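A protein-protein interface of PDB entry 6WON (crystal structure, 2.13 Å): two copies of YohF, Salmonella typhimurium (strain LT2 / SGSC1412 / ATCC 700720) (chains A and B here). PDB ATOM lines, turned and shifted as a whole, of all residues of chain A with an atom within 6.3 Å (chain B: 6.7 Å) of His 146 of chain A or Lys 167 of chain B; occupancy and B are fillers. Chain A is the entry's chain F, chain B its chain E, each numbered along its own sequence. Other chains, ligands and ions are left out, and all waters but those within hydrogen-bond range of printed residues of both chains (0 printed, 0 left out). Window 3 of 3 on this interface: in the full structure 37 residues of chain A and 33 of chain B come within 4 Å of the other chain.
OG of Ser 168 of chain B touches CB of Pro 148 of chain A, at 3.6 Å.
Leu 171 of chain B touches Pro 148 of chain A.
Gly 164 of chain B touches Thr 156 of chain A.
Gly 164 of chain B touches His 160 of chain A (CA to CD2, 3.3 Å).
The side-chain amino group of Lys 167 of chain B lies within hydrogen-bond range of the backbone carbonyl oxygen of His 146 of chain A, 2.8 Å away.
The side-chain amino group (NZ) of Lys 167 of chain B sits at hydrogen-bond distance from a ring nitrogen (NE2) of His 160 of chain A (3.0 Å).
The side-chain hydroxyl of Ser 168 of chain B sits close to the side-chain hydroxyl of Thr 156 of chain A, at 3.4 Å.
Of the 18 printed residues of chain B, 4 touch a printed residue of chain A.
Printed residues of chain B that touch a printed residue of chain A: Gly 164, Lys 167, Ser 168 and Leu 171.
Of the 16 printed residues of chain A, 4 touch a printed residue of chain B.
Printed residues of chain A that touch a printed residue of chain B: His 146, Pro 148, Thr 156 and His 160.
Hydrophobic or aromatic side chains of chain A that line the printed part of chain B: Pro 148 and His 160.
Among the printed residues, no Asp or Glu carboxylate lies within 4 Å of a Lys or Arg side-chain nitrogen of the other chain.
His 144 of chain A touches none of the printed residues of chain B.
His 146 of chain A touches just one residue of chain B: Lys 167 (2.8 Å).
Glu 145 of chain B touches none of the printed residues of chain A.
Lys 167 of chain B touches two residues of chain A.
Of the printed residues of chain A, Ser 168 of chain B touches Pro 148 (3.6 Å) and Thr 156 (3.3 Å).
Printed residues of chain A within 4 Å of Leu 171 of chain B: Pro 148.
The nearest residue of chain A that does not touch Lys 167 of chain B is Pro 148 of chain A (4.1 Å).
The nearest printed residue of chain B that does not touch His 160 of chain A is Gly 163 of chain B (4.2 Å).
A ring nitrogen (ND1) of His 160 of chain A is in hydrogen-bond range of the backbone carbonyl oxygen of His 144 of chain A, 3.0 Å away.
The side-chain carboxylate of Glu 145 of chain A sits close to a ring nitrogen (NE2) of His 146 of chain A (3.5 Å).
The backbone carbonyl oxygen (O) of Glu 145 of chain A lies close to a ring nitrogen (NE2) of His 160 of chain A (3.1 Å).
A ring nitrogen (NE2) of His 146 of chain A sits at hydrogen-bond distance from the side-chain hydroxyl of Ser 238 of chain A (2.8 Å).
The backbone carbonyl oxygen (O) of Thr 156 of chain A is in hydrogen-bond range of a ring nitrogen (ND1) of His 160 of chain A.
3 positions are printed for both chains.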
ATOM      1  N   THR A 141     -24.555 -12.078  10.828  1.00  0.00           N
ATOM      2  CA  THR A 141     -23.961 -11.948   9.503  1.00  0.00           C
ATOM      3  C   THR A 141     -24.982 -11.420   8.500  1.00  0.00           C
ATOM      4  O   THR A 141     -25.358 -10.242   8.558  1.00  0.00           O
ATOM      5  CB  THR A 141     -23.387 -13.283   9.032  1.00  0.00           C
ATOM      6  OG1 THR A 141     -24.431 -14.264   8.947  1.00  0.00           O
ATOM      7  CG2 THR A 141     -22.319 -13.761  10.012  1.00  0.00           C
ATOM      8  N   SER A 142     -25.460 -12.289   7.606  1.00  0.00           N
ATOM      9  CA  SER A 142     -26.286 -11.883   6.472  1.00  0.00           C
ATOM     10  C   SER A 142     -26.509 -13.082   5.575  1.00  0.00           C
ATOM     11  O   SER A 142     -25.709 -14.027   5.615  1.00  0.00           O
ATOM     12  CB  SER A 142     -25.606 -10.765   5.663  1.00  0.00           C
ATOM     13  OG  SER A 142     -26.307 -10.474   4.474  1.00  0.00           O
ATOM     14  N   VAL A 143     -27.578 -13.064   4.764  1.00  0.00           N
ATOM     15  CA  VAL A 143     -27.672 -14.060   3.708  1.00  0.00           C
ATOM     16  C   VAL A 143     -26.446 -13.998   2.816  1.00  0.00           C
ATOM     17  O   VAL A 143     -26.087 -14.988   2.170  1.00  0.00           O
ATOM     18  CB  VAL A 143     -28.943 -13.887   2.845  1.00  0.00           C
ATOM     19  CG1 VAL A 143     -30.171 -14.320   3.623  1.00  0.00           C
ATOM     20  CG2 VAL A 143     -29.054 -12.443   2.302  1.00  0.00           C
ATOM     21  N   HIS A 144     -25.813 -12.854   2.809  1.00  0.00           N
ATOM     22  CA  HIS A 144     -24.640 -12.619   2.054  1.00  0.00           C
ATOM     23  C   HIS A 144     -23.385 -13.355   2.546  1.00  0.00           C
ATOM     24  O   HIS A 144     -22.358 -13.262   1.963  1.00  0.00           O
ATOM     25  CB  HIS A 144     -24.519 -11.184   1.705  1.00  0.00           C
ATOM     26  CG  HIS A 144     -25.679 -10.713   0.930  1.00  0.00           C
ATOM     27  ND1 HIS A 144     -25.922 -11.135  -0.344  1.00  0.00           N
ATOM     28  CD2 HIS A 144     -26.723  -9.944   1.274  1.00  0.00           C
ATOM     29  CE1 HIS A 144     -27.041 -10.607  -0.766  1.00  0.00           C
ATOM     30  NE2 HIS A 144     -27.543  -9.876   0.195  1.00  0.00           N
ATOM     31  N   GLU A 145     -23.490 -13.933   3.721  1.00  0.00           N
ATOM     32  CA  GLU A 145     -22.507 -14.920   4.151  1.00  0.00           C
ATOM     33  C   GLU A 145     -22.481 -16.108   3.193  1.00  0.00           C
ATOM     34  O   GLU A 145     -21.503 -16.866   3.176  1.00  0.00           O
ATOM     35  CB  GLU A 145     -22.837 -15.373   5.590  1.00  0.00           C
ATOM     36  CG  GLU A 145     -21.916 -16.454   6.178  1.00  0.00           C
ATOM     37  CD  GLU A 145     -22.504 -17.160   7.398  1.00  0.00           C
ATOM     38  OE1 GLU A 145     -23.385 -16.582   8.079  1.00  0.00           O
ATOM     39  OE2 GLU A 145     -22.076 -18.307   7.673  1.00  0.00           O
ATOM     40  N   HIS A 146     -23.517 -16.262   2.367  1.00  0.00           N
ATOM     41  CA  HIS A 146     -23.695 -17.477   1.577  1.00  0.00           C
ATOM     42  C   HIS A 146     -23.853 -17.225   0.081  1.00  0.00           C
ATOM     43  O   HIS A 146     -23.509 -18.084  -0.737  1.00  0.00           O
ATOM     44  CB  HIS A 146     -24.914 -18.246   2.108  1.00  0.00           C
ATOM     45  CG  HIS A 146     -24.835 -18.547   3.572  1.00  0.00           C
ATOM     46  ND1 HIS A 146     -24.034 -19.551   4.082  1.00  0.00           N
ATOM     47  CD2 HIS A 146     -25.438 -17.968   4.637  1.00  0.00           C
ATOM     48  CE1 HIS A 146     -24.151 -19.578   5.401  1.00  0.00           C
ATOM     49  NE2 HIS A 146     -24.993 -18.625   5.763  1.00  0.00           N
ATOM     50  N   THR A 147     -24.376 -16.062  -0.295  1.00  0.00           N
ATOM     51  CA  THR A 147     -24.679 -15.754  -1.683  1.00  0.00           C
ATOM     52  C   THR A 147     -24.289 -14.296  -1.910  1.00  0.00           C
ATOM     53  O   THR A 147     -24.404 -13.485  -0.986  1.00  0.00           O
ATOM     54  CB  THR A 147     -26.174 -15.993  -1.986  1.00  0.00           C
ATOM     55  OG1 THR A 147     -26.451 -15.730  -3.374  1.00  0.00           O
ATOM     56  CG2 THR A 147     -27.048 -15.106  -1.122  1.00  0.00           C
ATOM     57  N   PRO A 148     -23.785 -13.936  -3.087  1.00  0.00           N
ATOM     58  CA  PRO A 148     -23.221 -12.587  -3.255  1.00  0.00           C
ATOM     59  C   PRO A 148     -24.281 -11.493  -3.318  1.00  0.00           C
ATOM     60  O   PRO A 148     -25.386 -11.692  -3.823  1.00  0.00           O
ATOM     61  CB  PRO A 148     -22.468 -12.684  -4.583  1.00  0.00           C
ATOM     62  CG  PRO A 148     -23.238 -13.757  -5.359  1.00  0.00           C
ATOM     63  CD  PRO A 148     -23.630 -14.764  -4.305  1.00  0.00           C
ATOM     64  N   THR A 156     -19.859  -8.896   0.896  1.00  0.00           N
ATOM     65  CA  THR A 156     -20.009 -10.341   0.748  1.00  0.00           C
ATOM     66  C   THR A 156     -18.793 -11.077   1.299  1.00  0.00           C
ATOM     67  O   THR A 156     -18.929 -12.039   2.064  1.00  0.00           O
ATOM     68  CB  THR A 156     -20.240 -10.690  -0.726  1.00  0.00           C
ATOM     69  OG1 THR A 156     -21.398  -9.988  -1.200  1.00  0.00           O
ATOM     70  CG2 THR A 156     -20.449 -12.206  -0.900  1.00  0.00           C
ATOM     71  N   LYS A 159     -18.653 -10.844   5.189  1.00  0.00           N
ATOM     72  CA  LYS A 159     -19.670 -11.686   5.817  1.00  0.00           C
ATOM     73  C   LYS A 159     -19.292 -13.156   5.731  1.00  0.00           C
ATOM     74  O   LYS A 159     -19.529 -13.922   6.674  1.00  0.00           O
ATOM     75  CB  LYS A 159     -21.031 -11.467   5.155  1.00  0.00           C
ATOM     76  CG  LYS A 159     -21.573 -10.064   5.340  1.00  0.00           C
ATOM     77  CD  LYS A 159     -21.743  -9.731   6.815  1.00  0.00           C
ATOM     78  CE  LYS A 159     -22.927  -8.820   7.013  1.00  0.00           C
ATOM     79  NZ  LYS A 159     -22.897  -8.163   8.320  1.00  0.00           N
ATOM     80  N   HIS A 160     -18.750 -13.577   4.586  1.00  0.00           N
ATOM     81  CA  HIS A 160     -18.210 -14.927   4.480  1.00  0.00           C
ATOM     82  C   HIS A 160     -17.115 -15.140   5.522  1.00  0.00           C
ATOM     83  O   HIS A 160     -17.062 -16.189   6.178  1.00  0.00           O
ATOM     84  CB  HIS A 160     -17.658 -15.170   3.070  1.00  0.00           C
ATOM     85  CG  HIS A 160     -18.695 -15.560   2.058  1.00  0.00           C
ATOM     86  ND1 HIS A 160     -19.717 -14.719   1.668  1.00  0.00           N
ATOM     87  CD2 HIS A 160     -18.840 -16.695   1.325  1.00  0.00           C
ATOM     88  CE1 HIS A 160     -20.458 -15.326   0.755  1.00  0.00           C
ATOM     89  NE2 HIS A 160     -19.950 -16.527   0.528  1.00  0.00           N
ATOM     90  N   ALA A 184     -28.174 -15.068  10.196  1.00  0.00           N
ATOM     91  CA  ALA A 184     -27.921 -14.473   8.889  1.00  0.00           C
ATOM     92  C   ALA A 184     -29.216 -13.883   8.345  1.00  0.00           C
ATOM     93  O   ALA A 184     -30.012 -14.588   7.706  1.00  0.00           O
ATOM     94  CB  ALA A 184     -27.351 -15.523   7.932  1.00  0.00           C
ATOM     95  N   SER A 238     -25.035 -21.462  10.923  1.00  0.00           N
ATOM     96  CA  SER A 238     -25.477 -20.178  10.386  1.00  0.00           C
ATOM     97  C   SER A 238     -26.979 -20.279  10.159  1.00  0.00           C
ATOM     98  O   SER A 238     -27.419 -20.953   9.226  1.00  0.00           O
ATOM     99  CB  SER A 238     -24.746 -19.832   9.090  1.00  0.00           C
ATOM    100  OG  SER A 238     -25.231 -18.616   8.541  1.00  0.00           O
ATOM    101  N   LEU A 239     -27.764 -19.622  11.014  1.00  0.00           N
ATOM    102  CA  LEU A 239     -29.218 -19.770  11.020  1.00  0.00           C
ATOM    103  C   LEU A 239     -29.817 -18.631  10.198  1.00  0.00           C
ATOM    104  O   LEU A 239     -29.723 -17.463  10.587  1.00  0.00           O
ATOM    105  CB  LEU A 239     -29.747 -19.768  12.454  1.00  0.00           C
ATOM    106  CG  LEU A 239     -29.111 -20.762  13.434  1.00  0.00           C
ATOM    107  CD1 LEU A 239     -29.908 -20.814  14.750  1.00  0.00           C
ATOM    108  CD2 LEU A 239     -29.042 -22.135  12.805  1.00  0.00           C
ATOM    109  N   ILE A 240     -30.421 -18.965   9.060  1.00  0.00           N
ATOM    110  CA  ILE A 240     -30.806 -17.972   8.063  1.00  0.00           C
ATOM    111  C   ILE A 240     -32.265 -17.601   8.271  1.00  0.00           C
ATOM    112  O   ILE A 240     -33.150 -18.470   8.275  1.00  0.00           O
ATOM    113  CB  ILE A 240     -30.553 -18.486   6.637  1.00  0.00           C
ATOM    114  CG1 ILE A 240     -29.045 -18.635   6.393  1.00  0.00           C
ATOM    115  CG2 ILE A 240     -31.165 -17.537   5.611  1.00  0.00           C
ATOM    116  CD1 ILE A 240     -28.687 -19.473   5.120  1.00  0.00           C
ATOM    117  N   MET A 246     -33.093 -17.180   0.100  1.00  0.00           N
ATOM    118  CA  MET A 246     -32.195 -18.222  -0.401  1.00  0.00           C
ATOM    119  C   MET A 246     -32.876 -19.196  -1.363  1.00  0.00           C
ATOM    120  O   MET A 246     -32.177 -19.931  -2.067  1.00  0.00           O
ATOM    121  CB  MET A 246     -31.594 -19.037   0.761  1.00  0.00           C
ATOM    122  CG  MET A 246     -30.650 -18.285   1.699  1.00  0.00           C
ATOM    123  SD  MET A 246     -29.260 -17.431   0.944  1.00  0.00           S
ATOM    124  CE  MET A 246     -28.421 -18.750   0.048  1.00  0.00           C
ATOM    125  N   ASN B 139      -9.285 -18.796  -8.130  1.00  0.00           N
ATOM    126  CA  ASN B 139      -8.785 -18.583  -6.773  1.00  0.00           C
ATOM    127  C   ASN B 139      -8.547 -19.941  -6.121  1.00  0.00           C
ATOM    128  O   ASN B 139      -9.491 -20.708  -5.928  1.00  0.00           O
ATOM    129  CB  ASN B 139      -9.771 -17.755  -5.947  1.00  0.00           C
ATOM    130  CG  ASN B 139      -9.977 -16.362  -6.517  1.00  0.00           C
ATOM    131  OD1 ASN B 139      -9.023 -15.713  -6.958  1.00  0.00           O
ATOM    132  ND2 ASN B 139     -11.228 -15.901  -6.532  1.00  0.00           N
ATOM    133  N   GLU B 145     -12.181 -23.163   3.074  1.00  0.00           N
ATOM    134  CA  GLU B 145     -13.220 -22.248   2.611  1.00  0.00           C
ATOM    135  C   GLU B 145     -14.602 -22.694   3.085  1.00  0.00           C
ATOM    136  O   GLU B 145     -15.529 -21.875   3.140  1.00  0.00           O
ATOM    137  CB  GLU B 145     -13.188 -22.166   1.076  1.00  0.00           C
ATOM    138  CG  GLU B 145     -14.185 -21.191   0.428  1.00  0.00           C
ATOM    139  CD  GLU B 145     -14.439 -21.496  -1.053  1.00  0.00           C
ATOM    140  OE1 GLU B 145     -13.548 -22.057  -1.727  1.00  0.00           O
ATOM    141  OE2 GLU B 145     -15.545 -21.188  -1.542  1.00  0.00           O
ATOM    142  N   HIS B 146     -14.758 -23.973   3.442  1.00  0.00           N
ATOM    143  CA  HIS B 146     -16.065 -24.517   3.781  1.00  0.00           C
ATOM    144  C   HIS B 146     -16.173 -25.078   5.191  1.00  0.00           C
ATOM    145  O   HIS B 146     -17.292 -25.162   5.715  1.00  0.00           O
ATOM    146  CB  HIS B 146     -16.454 -25.617   2.776  1.00  0.00           C
ATOM    147  CG  HIS B 146     -16.308 -25.194   1.350  1.00  0.00           C
ATOM    148  ND1 HIS B 146     -17.232 -24.389   0.716  1.00  0.00           N
ATOM    149  CD2 HIS B 146     -15.326 -25.425   0.446  1.00  0.00           C
ATOM    150  CE1 HIS B 146     -16.835 -24.160  -0.523  1.00  0.00           C
ATOM    151  NE2 HIS B 146     -15.680 -24.776  -0.711  1.00  0.00           N
ATOM    152  N   LEU B 162     -12.229 -15.382   0.763  1.00  0.00           N
ATOM    153  CA  LEU B 162     -11.877 -15.540  -0.643  1.00  0.00           C
ATOM    154  C   LEU B 162     -12.949 -16.325  -1.396  1.00  0.00           C
ATOM    155  O   LEU B 162     -13.196 -16.059  -2.580  1.00  0.00           O
ATOM    156  CB  LEU B 162     -10.503 -16.212  -0.773  1.00  0.00           C
ATOM    157  CG  LEU B 162      -9.909 -16.360  -2.177  1.00  0.00           C
ATOM    158  CD1 LEU B 162      -9.947 -15.025  -2.928  1.00  0.00           C
ATOM    159  CD2 LEU B 162      -8.474 -16.894  -2.084  1.00  0.00           C
ATOM    160  N   GLY B 163     -13.607 -17.273  -0.732  1.00  0.00           N
ATOM    161  CA  GLY B 163     -14.737 -17.946  -1.359  1.00  0.00           C
ATOM    162  C   GLY B 163     -15.872 -16.994  -1.698  1.00  0.00           C
ATOM    163  O   GLY B 163     -16.462 -17.077  -2.781  1.00  0.00           O
ATOM    164  N   GLY B 164     -16.198 -16.080  -0.777  1.00  0.00           N
ATOM    165  CA  GLY B 164     -17.225 -15.091  -1.066  1.00  0.00           C
ATOM    166  C   GLY B 164     -16.808 -14.106  -2.144  1.00  0.00           C
ATOM    167  O   GLY B 164     -17.621 -13.715  -2.991  1.00  0.00           O
ATOM    168  N   LEU B 165     -15.536 -13.691  -2.133  1.00  0.00           N
ATOM    169  CA  LEU B 165     -15.036 -12.824  -3.199  1.00  0.00           C
ATOM    170  C   LEU B 165     -15.158 -13.504  -4.560  1.00  0.00           C
ATOM    171  O   LEU B 165     -15.508 -12.859  -5.559  1.00  0.00           O
ATOM    172  CB  LEU B 165     -13.576 -12.436  -2.928  1.00  0.00           C
ATOM    173  CG  LEU B 165     -12.856 -11.603  -4.007  1.00  0.00           C
ATOM    174  CD1 LEU B 165     -13.481 -10.207  -4.137  1.00  0.00           C
ATOM    175  CD2 LEU B 165     -11.372 -11.482  -3.704  1.00  0.00           C
ATOM    176  N   THR B 166     -14.846 -14.799  -4.622  1.00  0.00           N
ATOM    177  CA  THR B 166     -15.000 -15.545  -5.866  1.00  0.00           C
ATOM    178  C   THR B 166     -16.415 -15.402  -6.412  1.00  0.00           C
ATOM    179  O   THR B 166     -16.613 -15.113  -7.597  1.00  0.00           O
ATOM    180  CB  THR B 166     -14.655 -17.018  -5.635  1.00  0.00           C
ATOM    181  OG1 THR B 166     -13.303 -17.121  -5.188  1.00  0.00           O
ATOM    182  CG2 THR B 166     -14.812 -17.823  -6.916  1.00  0.00           C
ATOM    183  N   LYS B 167     -17.414 -15.579  -5.544  1.00  0.00           N
ATOM    184  CA  LYS B 167     -18.807 -15.455  -5.963  1.00  0.00           C
ATOM    185  C   LYS B 167     -19.122 -14.055  -6.485  1.00  0.00           C
ATOM    186  O   LYS B 167     -19.788 -13.904  -7.515  1.00  0.00           O
ATOM    187  CB  LYS B 167     -19.722 -15.798  -4.792  1.00  0.00           C
ATOM    188  CG  LYS B 167     -19.578 -17.234  -4.266  1.00  0.00           C
ATOM    189  CD  LYS B 167     -20.400 -17.416  -2.988  1.00  0.00           C
ATOM    190  CE  LYS B 167     -20.137 -18.764  -2.343  1.00  0.00           C
ATOM    191  NZ  LYS B 167     -20.873 -18.878  -1.049  1.00  0.00           N
ATOM    192  N   SER B 168     -18.674 -13.019  -5.767  1.00  0.00           N
ATOM    193  CA  SER B 168     -18.972 -11.648  -6.176  1.00  0.00           C
ATOM    194  C   SER B 168     -18.268 -11.290  -7.486  1.00  0.00           C
ATOM    195  O   SER B 168     -18.855 -10.620  -8.348  1.00  0.00           O
ATOM    196  CB  SER B 168     -18.566 -10.678  -5.064  1.00  0.00           C
ATOM    197  OG  SER B 168     -19.502 -10.686  -3.990  1.00  0.00           O
ATOM    198  N   MET B 169     -17.005 -11.710  -7.643  1.00  0.00           N
ATOM    199  CA  MET B 169     -16.289 -11.470  -8.897  1.00  0.00           C
ATOM    200  C   MET B 169     -16.977 -12.165 -10.063  1.00  0.00           C
ATOM    201  O   MET B 169     -17.087 -11.600 -11.154  1.00  0.00           O
ATOM    202  CB  MET B 169     -14.841 -11.948  -8.787  1.00  0.00           C
ATOM    203  CG  MET B 169     -13.980 -11.159  -7.823  1.00  0.00           C
ATOM    204  SD  MET B 169     -12.320 -11.844  -7.702  1.00  0.00           S
ATOM    205  CE  MET B 169     -11.897 -11.908  -9.450  1.00  0.00           C
ATOM    206  N   ALA B 170     -17.437 -13.401  -9.858  1.00  0.00           N
ATOM    207  CA  ALA B 170     -18.100 -14.114 -10.939  1.00  0.00           C
ATOM    208  C   ALA B 170     -19.362 -13.383 -11.378  1.00  0.00           C
ATOM    209  O   ALA B 170     -19.624 -13.243 -12.580  1.00  0.00           O
ATOM    210  CB  ALA B 170     -18.409 -15.554 -10.505  1.00  0.00           C
ATOM    211  N   LEU B 171     -20.138 -12.884 -10.417  1.00  0.00           N
ATOM    212  CA  LEU B 171     -21.380 -12.194 -10.739  1.00  0.00           C
ATOM    213  C   LEU B 171     -21.125 -10.872 -11.463  1.00  0.00           C
ATOM    214  O   LEU B 171     -21.803 -10.562 -12.453  1.00  0.00           O
ATOM    215  CB  LEU B 171     -22.180 -11.964  -9.457  1.00  0.00           C
ATOM    216  CG  LEU B 171     -23.639 -11.535  -9.617  1.00  0.00           C
ATOM    217  CD1 LEU B 171     -24.433 -12.588 -10.398  1.00  0.00           C
ATOM    218  CD2 LEU B 171     -24.275 -11.301  -8.261  1.00  0.00           C
ATOM    219  N   GLU B 172     -20.153 -10.081 -10.990  1.00  0.00           N
ATOM    220  CA  GLU B 172     -19.920  -8.754 -11.558  1.00  0.00           C
ATOM    221  C   GLU B 172     -19.121  -8.784 -12.856  1.00  0.00           C
ATOM    222  O   GLU B 172     -19.243  -7.849 -13.658  1.00  0.00           O
ATOM    223  CB  GLU B 172     -19.205  -7.855 -10.543  1.00  0.00           C
ATOM    224  CG  GLU B 172     -20.038  -7.606  -9.279  1.00  0.00           C
ATOM    225  CD  GLU B 172     -19.479  -6.504  -8.372  1.00  0.00           C
ATOM    226  OE1 GLU B 172     -18.763  -5.608  -8.865  1.00  0.00           O
ATOM    227  OE2 GLU B 172     -19.771  -6.545  -7.155  1.00  0.00           O
ATOM    228  N   VAL B 180     -15.071 -16.839 -13.076  1.00  0.00           N
ATOM    229  CA  VAL B 180     -14.320 -16.839 -11.828  1.00  0.00           C
ATOM    230  C   VAL B 180     -14.765 -18.035 -10.994  1.00  0.00           C
ATOM    231  O   VAL B 180     -15.964 -18.211 -10.736  1.00  0.00           O
ATOM    232  CB  VAL B 180     -14.506 -15.520 -11.047  1.00  0.00           C
ATOM    233  CG1 VAL B 180     -13.586 -15.470  -9.816  1.00  0.00           C
ATOM    234  CG2 VAL B 180     -14.247 -14.310 -11.955  1.00  0.00           C
ATOM    235  N   GLY B 236     -18.552 -19.019 -10.733  1.00  0.00           N
ATOM    236  CA  GLY B 236     -19.108 -18.794  -9.411  1.00  0.00           C
ATOM    237  C   GLY B 236     -19.007 -19.949  -8.433  1.00  0.00           C
ATOM    238  O   GLY B 236     -19.594 -19.862  -7.343  1.00  0.00           O
ATOM    239  N   GLN B 237     -18.271 -21.013  -8.764  1.00  0.00           N
ATOM    240  CA  GLN B 237     -18.310 -22.249  -7.995  1.00  0.00           C
ATOM    241  C   GLN B 237     -16.999 -22.495  -7.248  1.00  0.00           C
ATOM    242  O   GLN B 237     -15.934 -21.996  -7.620  1.00  0.00           O
ATOM    243  CB  GLN B 237     -18.628 -23.431  -8.913  1.00  0.00           C
ATOM    244  CG  GLN B 237     -20.118 -23.511  -9.288  1.00  0.00           C
ATOM    245  CD  GLN B 237     -20.985 -23.702  -8.056  1.00  0.00           C
ATOM    246  OE1 GLN B 237     -20.717 -24.589  -7.236  1.00  0.00           O
ATOM    247  NE2 GLN B 237     -22.012 -22.857  -7.895  1.00  0.00           N
ATOM    248  N   SER B 238     -17.088 -23.287  -6.180  1.00  0.00           N
ATOM    249  CA  SER B 238     -15.919 -23.752  -5.447  1.00  0.00           C
ATOM    250  C   SER B 238     -15.800 -25.262  -5.675  1.00  0.00           C
ATOM    251  O   SER B 238     -16.585 -26.041  -5.128  1.00  0.00           O
ATOM    252  CB  SER B 238     -16.038 -23.390  -3.962  1.00  0.00           C
ATOM    253  OG  SER B 238     -14.895 -23.816  -3.224  1.00  0.00           O
